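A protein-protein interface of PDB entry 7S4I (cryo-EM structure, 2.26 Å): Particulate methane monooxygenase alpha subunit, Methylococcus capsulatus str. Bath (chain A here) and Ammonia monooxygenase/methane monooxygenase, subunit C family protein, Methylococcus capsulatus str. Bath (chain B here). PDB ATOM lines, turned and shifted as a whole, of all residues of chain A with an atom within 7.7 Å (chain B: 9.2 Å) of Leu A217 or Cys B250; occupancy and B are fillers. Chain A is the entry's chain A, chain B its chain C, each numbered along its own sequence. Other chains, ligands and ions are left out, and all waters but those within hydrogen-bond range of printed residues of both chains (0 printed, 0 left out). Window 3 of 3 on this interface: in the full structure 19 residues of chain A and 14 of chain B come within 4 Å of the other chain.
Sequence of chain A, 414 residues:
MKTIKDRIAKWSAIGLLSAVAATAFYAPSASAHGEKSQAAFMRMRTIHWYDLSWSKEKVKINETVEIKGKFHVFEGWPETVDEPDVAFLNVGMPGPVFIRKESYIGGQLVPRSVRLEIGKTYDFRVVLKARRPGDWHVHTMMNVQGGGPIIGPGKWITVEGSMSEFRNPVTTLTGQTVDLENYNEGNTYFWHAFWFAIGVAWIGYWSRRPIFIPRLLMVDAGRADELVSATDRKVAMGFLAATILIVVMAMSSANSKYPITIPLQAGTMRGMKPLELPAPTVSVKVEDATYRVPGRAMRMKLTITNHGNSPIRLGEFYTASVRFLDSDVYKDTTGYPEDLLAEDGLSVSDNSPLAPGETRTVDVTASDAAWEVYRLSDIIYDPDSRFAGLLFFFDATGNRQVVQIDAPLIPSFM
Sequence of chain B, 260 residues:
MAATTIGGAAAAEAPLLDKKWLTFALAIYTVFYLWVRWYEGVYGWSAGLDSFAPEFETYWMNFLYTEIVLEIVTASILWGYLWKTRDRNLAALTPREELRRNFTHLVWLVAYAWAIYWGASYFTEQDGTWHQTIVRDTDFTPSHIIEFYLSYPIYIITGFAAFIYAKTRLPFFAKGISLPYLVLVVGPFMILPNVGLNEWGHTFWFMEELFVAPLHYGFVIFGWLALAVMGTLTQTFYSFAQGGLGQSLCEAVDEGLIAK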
ATOM      1  N   PHE A 212       7.883 -21.040  14.165  1.00  0.00           N
ATOM      2  CA  PHE A 212       7.514 -19.661  13.854  1.00  0.00           C
ATOM      3  C   PHE A 212       6.010 -19.412  13.789  1.00  0.00           C
ATOM      4  O   PHE A 212       5.477 -18.642  14.590  1.00  0.00           O
ATOM      5  CB  PHE A 212       8.172 -19.243  12.533  1.00  0.00           C
ATOM      6  CG  PHE A 212       9.631 -18.929  12.663  1.00  0.00           C
ATOM      7  CD1 PHE A 212      10.054 -17.855  13.426  1.00  0.00           C
ATOM      8  CD2 PHE A 212      10.581 -19.708  12.026  1.00  0.00           C
ATOM      9  CE1 PHE A 212      11.396 -17.563  13.551  1.00  0.00           C
ATOM     10  CE2 PHE A 212      11.925 -19.420  12.147  1.00  0.00           C
ATOM     11  CZ  PHE A 212      12.333 -18.347  12.910  1.00  0.00           C
ATOM     12  N   ILE A 213       5.306 -20.065  12.872  1.00  0.00           N
ATOM     13  CA  ILE A 213       3.943 -19.634  12.562  1.00  0.00           C
ATOM     14  C   ILE A 213       2.957 -20.108  13.627  1.00  0.00           C
ATOM     15  O   ILE A 213       2.137 -19.298  14.088  1.00  0.00           O
ATOM     16  CB  ILE A 213       3.514 -20.087  11.158  1.00  0.00           C
ATOM     17  CG1 ILE A 213       4.323 -19.344  10.093  1.00  0.00           C
ATOM     18  CG2 ILE A 213       2.042 -19.803  10.950  1.00  0.00           C
ATOM     19  CD1 ILE A 213       3.720 -19.403   8.707  1.00  0.00           C
ATOM     20  N   PRO A 214       2.956 -21.385  14.036  1.00  0.00           N
ATOM     21  CA  PRO A 214       2.049 -21.770  15.131  1.00  0.00           C
ATOM     22  C   PRO A 214       2.315 -21.023  16.426  1.00  0.00           C
ATOM     23  O   PRO A 214       1.363 -20.657  17.125  1.00  0.00           O
ATOM     24  CB  PRO A 214       2.292 -23.280  15.277  1.00  0.00           C
ATOM     25  CG  PRO A 214       3.600 -23.525  14.637  1.00  0.00           C
ATOM     26  CD  PRO A 214       3.688 -22.554  13.516  1.00  0.00           C
ATOM     27  N   ARG A 215       3.582 -20.763  16.761  1.00  0.00           N
ATOM     28  CA  ARG A 215       3.873 -20.007  17.975  1.00  0.00           C
ATOM     29  C   ARG A 215       3.401 -18.564  17.849  1.00  0.00           C
ATOM     30  O   ARG A 215       2.871 -17.992  18.810  1.00  0.00           O
ATOM     31  CB  ARG A 215       5.368 -20.060  18.295  1.00  0.00           C
ATOM     32  CG  ARG A 215       5.842 -21.409  18.807  1.00  0.00           C
ATOM     33  CD  ARG A 215       7.306 -21.384  19.201  1.00  0.00           C
ATOM     34  NE  ARG A 215       7.503 -20.909  20.565  1.00  0.00           N
ATOM     35  CZ  ARG A 215       7.576 -21.698  21.627  1.00  0.00           C
ATOM     36  NH1 ARG A 215       7.455 -23.011  21.523  1.00  0.00           N
ATOM     37  NH2 ARG A 215       7.778 -21.157  22.825  1.00  0.00           N
ATOM     38  N   LEU A 216       3.581 -17.962  16.671  1.00  0.00           N
ATOM     39  CA  LEU A 216       3.080 -16.612  16.440  1.00  0.00           C
ATOM     40  C   LEU A 216       1.566 -16.556  16.591  1.00  0.00           C
ATOM     41  O   LEU A 216       1.028 -15.636  17.218  1.00  0.00           O
ATOM     42  CB  LEU A 216       3.496 -16.139  15.049  1.00  0.00           C
ATOM     43  CG  LEU A 216       2.891 -14.838  14.521  1.00  0.00           C
ATOM     44  CD1 LEU A 216       3.459 -13.646  15.266  1.00  0.00           C
ATOM     45  CD2 LEU A 216       3.130 -14.707  13.027  1.00  0.00           C
ATOM     46  N   LEU A 217       0.865 -17.540  16.021  1.00  0.00           N
ATOM     47  CA  LEU A 217      -0.589 -17.576  16.131  1.00  0.00           C
ATOM     48  C   LEU A 217      -1.031 -17.782  17.575  1.00  0.00           C
ATOM     49  O   LEU A 217      -2.011 -17.176  18.019  1.00  0.00           O
ATOM     50  CB  LEU A 217      -1.157 -18.676  15.235  1.00  0.00           C
ATOM     51  CG  LEU A 217      -1.080 -18.426  13.729  1.00  0.00           C
ATOM     52  CD1 LEU A 217      -1.513 -19.662  12.960  1.00  0.00           C
ATOM     53  CD2 LEU A 217      -1.921 -17.226  13.338  1.00  0.00           C
ATOM     54  N   MET A 218      -0.329 -18.639  18.318  1.00  0.00           N
ATOM     55  CA  MET A 218      -0.669 -18.850  19.721  1.00  0.00           C
ATOM     56  C   MET A 218      -0.466 -17.581  20.538  1.00  0.00           C
ATOM     57  O   MET A 218      -1.292 -17.254  21.398  1.00  0.00           O
ATOM     58  CB  MET A 218       0.161 -19.996  20.296  1.00  0.00           C
ATOM     59  CG  MET A 218      -0.294 -21.373  19.850  1.00  0.00           C
ATOM     60  SD  MET A 218      -1.761 -21.926  20.734  1.00  0.00           S
ATOM     61  CE  MET A 218      -1.103 -22.105  22.389  1.00  0.00           C
ATOM     62  N   VAL A 219       0.628 -16.859  20.290  1.00  0.00           N
ATOM     63  CA  VAL A 219       0.879 -15.626  21.031  1.00  0.00           C
ATOM     64  C   VAL A 219      -0.156 -14.565  20.678  1.00  0.00           C
ATOM     65  O   VAL A 219      -0.660 -13.855  21.557  1.00  0.00           O
ATOM     66  CB  VAL A 219       2.313 -15.129  20.775  1.00  0.00           C
ATOM     67  CG1 VAL A 219       2.505 -13.740  21.357  1.00  0.00           C
ATOM     68  CG2 VAL A 219       3.323 -16.094  21.374  1.00  0.00           C
ATOM     69  N   ASP A 220      -0.499 -14.442  19.394  1.00  0.00           N
ATOM     70  CA  ASP A 220      -1.451 -13.414  18.968  1.00  0.00           C
ATOM     71  C   ASP A 220      -2.861 -13.720  19.461  1.00  0.00           C
ATOM     72  O   ASP A 220      -3.473 -12.918  20.175  1.00  0.00           O
ATOM     73  CB  ASP A 220      -1.428 -13.278  17.442  1.00  0.00           C
ATOM     74  CG  ASP A 220      -0.166 -12.613  16.934  1.00  0.00           C
ATOM     75  OD1 ASP A 220       0.335 -11.688  17.608  1.00  0.00           O
ATOM     76  OD2 ASP A 220       0.323 -13.010  15.857  1.00  0.00           O
ATOM     77  N   ALA A 221      -3.395 -14.882  19.087  1.00  0.00           N
ATOM     78  CA  ALA A 221      -4.761 -15.242  19.444  1.00  0.00           C
ATOM     79  C   ALA A 221      -4.844 -15.653  20.907  1.00  0.00           C
ATOM     80  O   ALA A 221      -4.625 -16.821  21.245  1.00  0.00           O
ATOM     81  CB  ALA A 221      -5.274 -16.366  18.542  1.00  0.00           C
ATOM     82  N   GLY A 222      -5.160 -14.699  21.776  1.00  0.00           N
ATOM     83  CA  GLY A 222      -5.254 -14.965  23.194  1.00  0.00           C
ATOM     84  C   GLY A 222      -3.896 -15.004  23.864  1.00  0.00           C
ATOM     85  O   GLY A 222      -2.843 -14.878  23.238  1.00  0.00           O
ATOM     86  N   ARG A 223      -3.933 -15.184  25.181  1.00  0.00           N
ATOM     87  CA  ARG A 223      -2.706 -15.329  25.946  1.00  0.00           C
ATOM     88  C   ARG A 223      -2.023 -16.641  25.576  1.00  0.00           C
ATOM     89  O   ARG A 223      -2.672 -17.667  25.360  1.00  0.00           O
ATOM     90  CB  ARG A 223      -3.011 -15.298  27.443  1.00  0.00           C
ATOM     91  CG  ARG A 223      -3.289 -13.912  27.992  1.00  0.00           C
ATOM     92  CD  ARG A 223      -3.742 -13.987  29.439  1.00  0.00           C
ATOM     93  NE  ARG A 223      -3.969 -12.666  30.011  1.00  0.00           N
ATOM     94  CZ  ARG A 223      -4.937 -12.384  30.872  1.00  0.00           C
ATOM     95  NH1 ARG A 223      -5.783 -13.312  31.290  1.00  0.00           N
ATOM     96  NH2 ARG A 223      -5.064 -11.138  31.320  1.00  0.00           N
ATOM     97  N   ALA A 224      -0.693 -16.605  25.491  1.00  0.00           N
ATOM     98  CA  ALA A 224      -0.009 -17.815  25.061  1.00  0.00           C
ATOM     99  C   ALA A 224       0.172 -18.779  26.223  1.00  0.00           C
ATOM    100  O   ALA A 224      -0.518 -19.801  26.290  1.00  0.00           O
ATOM    101  CB  ALA A 224       1.350 -17.465  24.452  1.00  0.00           C
ATOM    102  N   LEU A 227       3.322 -22.288  25.518  1.00  0.00           N
ATOM    103  CA  LEU A 227       4.502 -22.719  24.785  1.00  0.00           C
ATOM    104  C   LEU A 227       5.770 -22.655  25.621  1.00  0.00           C
ATOM    105  O   LEU A 227       6.808 -23.170  25.190  1.00  0.00           O
ATOM    106  CB  LEU A 227       4.666 -21.880  23.516  1.00  0.00           C
ATOM    107  CG  LEU A 227       3.360 -21.677  22.742  1.00  0.00           C
ATOM    108  CD1 LEU A 227       2.855 -20.260  22.917  1.00  0.00           C
ATOM    109  CD2 LEU A 227       3.503 -22.027  21.276  1.00  0.00           C
ATOM    110  N   THR B 234       7.493 -11.343   9.904  1.00  0.00           N
ATOM    111  CA  THR B 234       6.152 -11.508  10.462  1.00  0.00           C
ATOM    112  C   THR B 234       5.086 -11.122   9.440  1.00  0.00           C
ATOM    113  O   THR B 234       4.011 -11.738   9.402  1.00  0.00           O
ATOM    114  CB  THR B 234       5.984 -10.722  11.766  1.00  0.00           C
ATOM    115  OG1 THR B 234       4.616 -10.779  12.187  1.00  0.00           O
ATOM    116  CG2 THR B 234       6.375  -9.290  11.597  1.00  0.00           C
ATOM    117  N   PHE B 237       4.792 -14.145   7.323  1.00  0.00           N
ATOM    118  CA  PHE B 237       4.054 -15.169   8.053  1.00  0.00           C
ATOM    119  C   PHE B 237       2.555 -14.919   7.964  1.00  0.00           C
ATOM    120  O   PHE B 237       1.771 -15.848   7.734  1.00  0.00           O
ATOM    121  CB  PHE B 237       4.506 -15.203   9.512  1.00  0.00           C
ATOM    122  CG  PHE B 237       5.878 -15.769   9.707  1.00  0.00           C
ATOM    123  CD1 PHE B 237       6.427 -16.628   8.771  1.00  0.00           C
ATOM    124  CD2 PHE B 237       6.624 -15.437  10.824  1.00  0.00           C
ATOM    125  CE1 PHE B 237       7.692 -17.147   8.949  1.00  0.00           C
ATOM    126  CE2 PHE B 237       7.888 -15.953  11.006  1.00  0.00           C
ATOM    127  CZ  PHE B 237       8.422 -16.807  10.068  1.00  0.00           C
ATOM    128  N   TYR B 238       2.140 -13.664   8.140  1.00  0.00           N
ATOM    129  CA  TYR B 238       0.727 -13.331   7.991  1.00  0.00           C
ATOM    130  C   TYR B 238       0.248 -13.576   6.566  1.00  0.00           C
ATOM    131  O   TYR B 238      -0.873 -14.052   6.352  1.00  0.00           O
ATOM    132  CB  TYR B 238       0.480 -11.881   8.404  1.00  0.00           C
ATOM    133  CG  TYR B 238       0.491 -11.673   9.898  1.00  0.00           C
ATOM    134  CD1 TYR B 238      -0.021 -12.638  10.755  1.00  0.00           C
ATOM    135  CD2 TYR B 238       1.011 -10.514  10.453  1.00  0.00           C
ATOM    136  CE1 TYR B 238      -0.014 -12.455  12.121  1.00  0.00           C
ATOM    137  CE2 TYR B 238       1.023 -10.322  11.820  1.00  0.00           C
ATOM    138  CZ  TYR B 238       0.510 -11.295  12.648  1.00  0.00           C
ATOM    139  OH  TYR B 238       0.519 -11.104  14.010  1.00  0.00           O
ATOM    140  N   PHE B 240       1.475 -15.814   4.487  1.00  0.00           N
ATOM    141  CA  PHE B 240       1.354 -17.264   4.396  1.00  0.00           C
ATOM    142  C   PHE B 240       0.051 -17.740   5.017  1.00  0.00           C
ATOM    143  O   PHE B 240      -0.650 -18.584   4.445  1.00  0.00           O
ATOM    144  CB  PHE B 240       2.541 -17.923   5.099  1.00  0.00           C
ATOM    145  CG  PHE B 240       3.600 -18.439   4.170  1.00  0.00           C
ATOM    146  CD1 PHE B 240       3.376 -19.563   3.399  1.00  0.00           C
ATOM    147  CD2 PHE B 240       4.831 -17.810   4.087  1.00  0.00           C
ATOM    148  CE1 PHE B 240       4.355 -20.049   2.554  1.00  0.00           C
ATOM    149  CE2 PHE B 240       5.812 -18.287   3.243  1.00  0.00           C
ATOM    150  CZ  PHE B 240       5.574 -19.408   2.476  1.00  0.00           C
ATOM    151  N   ALA B 241      -0.287 -17.212   6.187  1.00  0.00           N
ATOM    152  CA  ALA B 241      -1.478 -17.617   6.931  1.00  0.00           C
ATOM    153  C   ALA B 241      -2.675 -16.734   6.601  1.00  0.00           C
ATOM    154  O   ALA B 241      -3.323 -16.190   7.494  1.00  0.00           O
ATOM    155  CB  ALA B 241      -1.182 -17.598   8.425  1.00  0.00           C
ATOM    156  N   GLN B 242      -2.990 -16.577   5.317  1.00  0.00           N
ATOM    157  CA  GLN B 242      -4.145 -15.763   4.913  1.00  0.00           C
ATOM    158  C   GLN B 242      -5.374 -16.640   4.703  1.00  0.00           C
ATOM    159  O   GLN B 242      -6.359 -16.532   5.439  1.00  0.00           O
ATOM    160  CB  GLN B 242      -3.813 -14.968   3.648  1.00  0.00           C
ATOM    161  CG  GLN B 242      -3.043 -13.668   3.869  1.00  0.00           C
ATOM    162  CD  GLN B 242      -3.849 -12.599   4.591  1.00  0.00           C
ATOM    163  OE1 GLN B 242      -4.350 -12.812   5.695  1.00  0.00           O
ATOM    164  NE2 GLN B 242      -3.980 -11.440   3.959  1.00  0.00           N
ATOM    165  N   GLY B 244      -4.815 -20.263   3.554  1.00  0.00           N
ATOM    166  CA  GLY B 244      -4.331 -21.584   3.894  1.00  0.00           C
ATOM    167  C   GLY B 244      -3.561 -21.603   5.196  1.00  0.00           C
ATOM    168  O   GLY B 244      -2.567 -22.324   5.327  1.00  0.00           O
ATOM    169  N   LEU B 245      -4.007 -20.804   6.166  1.00  0.00           N
ATOM    170  CA  LEU B 245      -3.379 -20.801   7.481  1.00  0.00           C
ATOM    171  C   LEU B 245      -3.477 -22.156   8.162  1.00  0.00           C
ATOM    172  O   LEU B 245      -2.677 -22.447   9.057  1.00  0.00           O
ATOM    173  CB  LEU B 245      -4.010 -19.715   8.361  1.00  0.00           C
ATOM    174  CG  LEU B 245      -5.332 -19.941   9.100  1.00  0.00           C
ATOM    175  CD1 LEU B 245      -5.103 -20.508  10.497  1.00  0.00           C
ATOM    176  CD2 LEU B 245      -6.135 -18.650   9.166  1.00  0.00           C
ATOM    177  N   GLY B 246      -4.438 -22.982   7.760  1.00  0.00           N
ATOM    178  CA  GLY B 246      -4.583 -24.316   8.297  1.00  0.00           C
ATOM    179  C   GLY B 246      -5.720 -25.043   7.614  1.00  0.00           C
ATOM    180  O   GLY B 246      -5.928 -24.923   6.405  1.00  0.00           O
ATOM    181  N   GLN B 247      -6.480 -25.778   8.416  1.00  0.00           N
ATOM    182  CA  GLN B 247      -6.288 -25.753   9.858  1.00  0.00           C
ATOM    183  C   GLN B 247      -5.426 -26.907  10.347  1.00  0.00           C
ATOM    184  O   GLN B 247      -5.049 -27.783   9.564  1.00  0.00           O
ATOM    185  CB  GLN B 247      -7.637 -25.759  10.572  1.00  0.00           C
ATOM    186  CG  GLN B 247      -8.441 -24.489  10.357  1.00  0.00           C
ATOM    187  CD  GLN B 247      -7.579 -23.242  10.422  1.00  0.00           C
ATOM    188  OE1 GLN B 247      -7.248 -22.650   9.396  1.00  0.00           O
ATOM    189  NE2 GLN B 247      -7.210 -22.840  11.632  1.00  0.00           N
ATOM    190  N   SER B 248      -5.216 -26.911  11.668  1.00  0.00           N
ATOM    191  CA  SER B 248      -4.126 -27.560  12.396  1.00  0.00           C
ATOM    192  C   SER B 248      -3.558 -26.525  13.353  1.00  0.00           C
ATOM    193  O   SER B 248      -3.783 -26.587  14.565  1.00  0.00           O
ATOM    194  CB  SER B 248      -3.010 -28.076  11.483  1.00  0.00           C
ATOM    195  OG  SER B 248      -1.807 -28.261  12.207  1.00  0.00           O
ATOM    196  N   LEU B 249      -2.804 -25.582  12.798  1.00  0.00           N
ATOM    197  CA  LEU B 249      -2.358 -24.405  13.530  1.00  0.00           C
ATOM    198  C   LEU B 249      -3.550 -23.706  14.167  1.00  0.00           C
ATOM    199  O   LEU B 249      -4.506 -23.337  13.476  1.00  0.00           O
ATOM    200  CB  LEU B 249      -1.620 -23.451  12.585  1.00  0.00           C
ATOM    201  CG  LEU B 249      -0.271 -23.804  11.936  1.00  0.00           C
ATOM    202  CD1 LEU B 249      -0.238 -25.153  11.226  1.00  0.00           C
ATOM    203  CD2 LEU B 249       0.106 -22.712  10.960  1.00  0.00           C
ATOM    204  N   CYS B 250      -3.489 -23.534  15.487  1.00  0.00           N
ATOM    205  CA  CYS B 250      -4.590 -22.971  16.270  1.00  0.00           C
ATOM    206  C   CYS B 250      -5.869 -23.789  16.085  1.00  0.00           C
ATOM    207  O   CYS B 250      -6.982 -23.257  16.054  1.00  0.00           O
ATOM    208  CB  CYS B 250      -4.821 -21.499  15.922  1.00  0.00           C
ATOM    209  SG  CYS B 250      -3.862 -20.339  16.923  1.00  0.00           S
ATOM    210  N   GLU B 251      -5.696 -25.102  15.960  1.00  0.00           N
ATOM    211  CA  GLU B 251      -6.816 -26.037  15.915  1.00  0.00           C
ATOM    212  C   GLU B 251      -6.341 -27.454  16.215  1.00  0.00           C
ATOM    213  O   GLU B 251      -6.183 -27.834  17.375  1.00  0.00           O
ATOM    214  CB  GLU B 251      -7.520 -26.002  14.556  1.00  0.00           C
ATOM    215  CG  GLU B 251      -9.027 -26.201  14.657  1.00  0.00           C
ATOM    216  CD  GLU B 251      -9.760 -25.858  13.376  1.00  0.00           C
ATOM    217  OE1 GLU B 251      -9.868 -26.742  12.500  1.00  0.00           O
ATOM    218  OE2 GLU B 251     -10.225 -24.708  13.242  1.00  0.00           O
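Hydrophobic or aromatic side chains of chain A within 4 Å of the printed part of chain B: Phe A212, Ile A213, Leu A216 and Leu A217.
Among the printed residues, 8 pairs touch across the chains.
Among the printed residues, no Asp or Glu carboxylate lies within 4 Å of a Lys or Arg side-chain nitrogen of the other chain.
Phe A212 touches Phe B237.
CG1 of Ile A213 touches CD1 of Phe B237, 3.7 Å away.
Leu B249 touches Ile A213 (CD2 to CG2, 3.5 Å).
Phe B237 touches Leu A216.
Tyr B238 touches Leu A216 (CE1 to CD2, 3.97 Å).
Leu A217 touches Leu B249.
CB of Leu A217 touches SG of Cys B250 (3.6 Å).
Leu A217 touches just these residues of chain B: Leu B249 and Cys B250.
Of chain A, only Leu A217 comes within 4 Å of Cys B250.
Of chain B, only Phe B237 (3.8 Å) and Tyr B238 (3.97 Å) come within 4 Å of Leu A216.
No residue of chain B comes within 4 Å of Ala A221.
Printed residues of chain B within 4 Å of Phe A212: Phe B237.
Of the printed residues of chain B, Ile A213 touches Phe B237 and Leu B249.
Printed residues of chain A within 4 Å of Leu B249: Ile A213 and Leu A217.
Of the printed residues of chain A, Phe B237 touches Phe A212 (3.5 Å), Ile A213 (3.7 Å) and Leu A216 (3.8 Å).
Of the printed residues of chain B, Asp A220 touches Tyr B238.
Gly B244 touches none of the printed residues of chain A.
The nearest residue of chain B that does not touch Leu A217 is Leu B245 (4.4 Å).
The nearest printed residue of chain A that does not touch Phe B237 is Leu A217 (6.9 Å).
The side-chain carboxylate of Asp A220 sits at hydrogen-bond distance from the side-chain hydroxyl of Tyr B238.
The side-chain amide nitrogen (NE2) of Gln B247 lies within hydrogen-bond range of the backbone carbonyl oxygen (O) of Leu B249 (3.3 Å).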
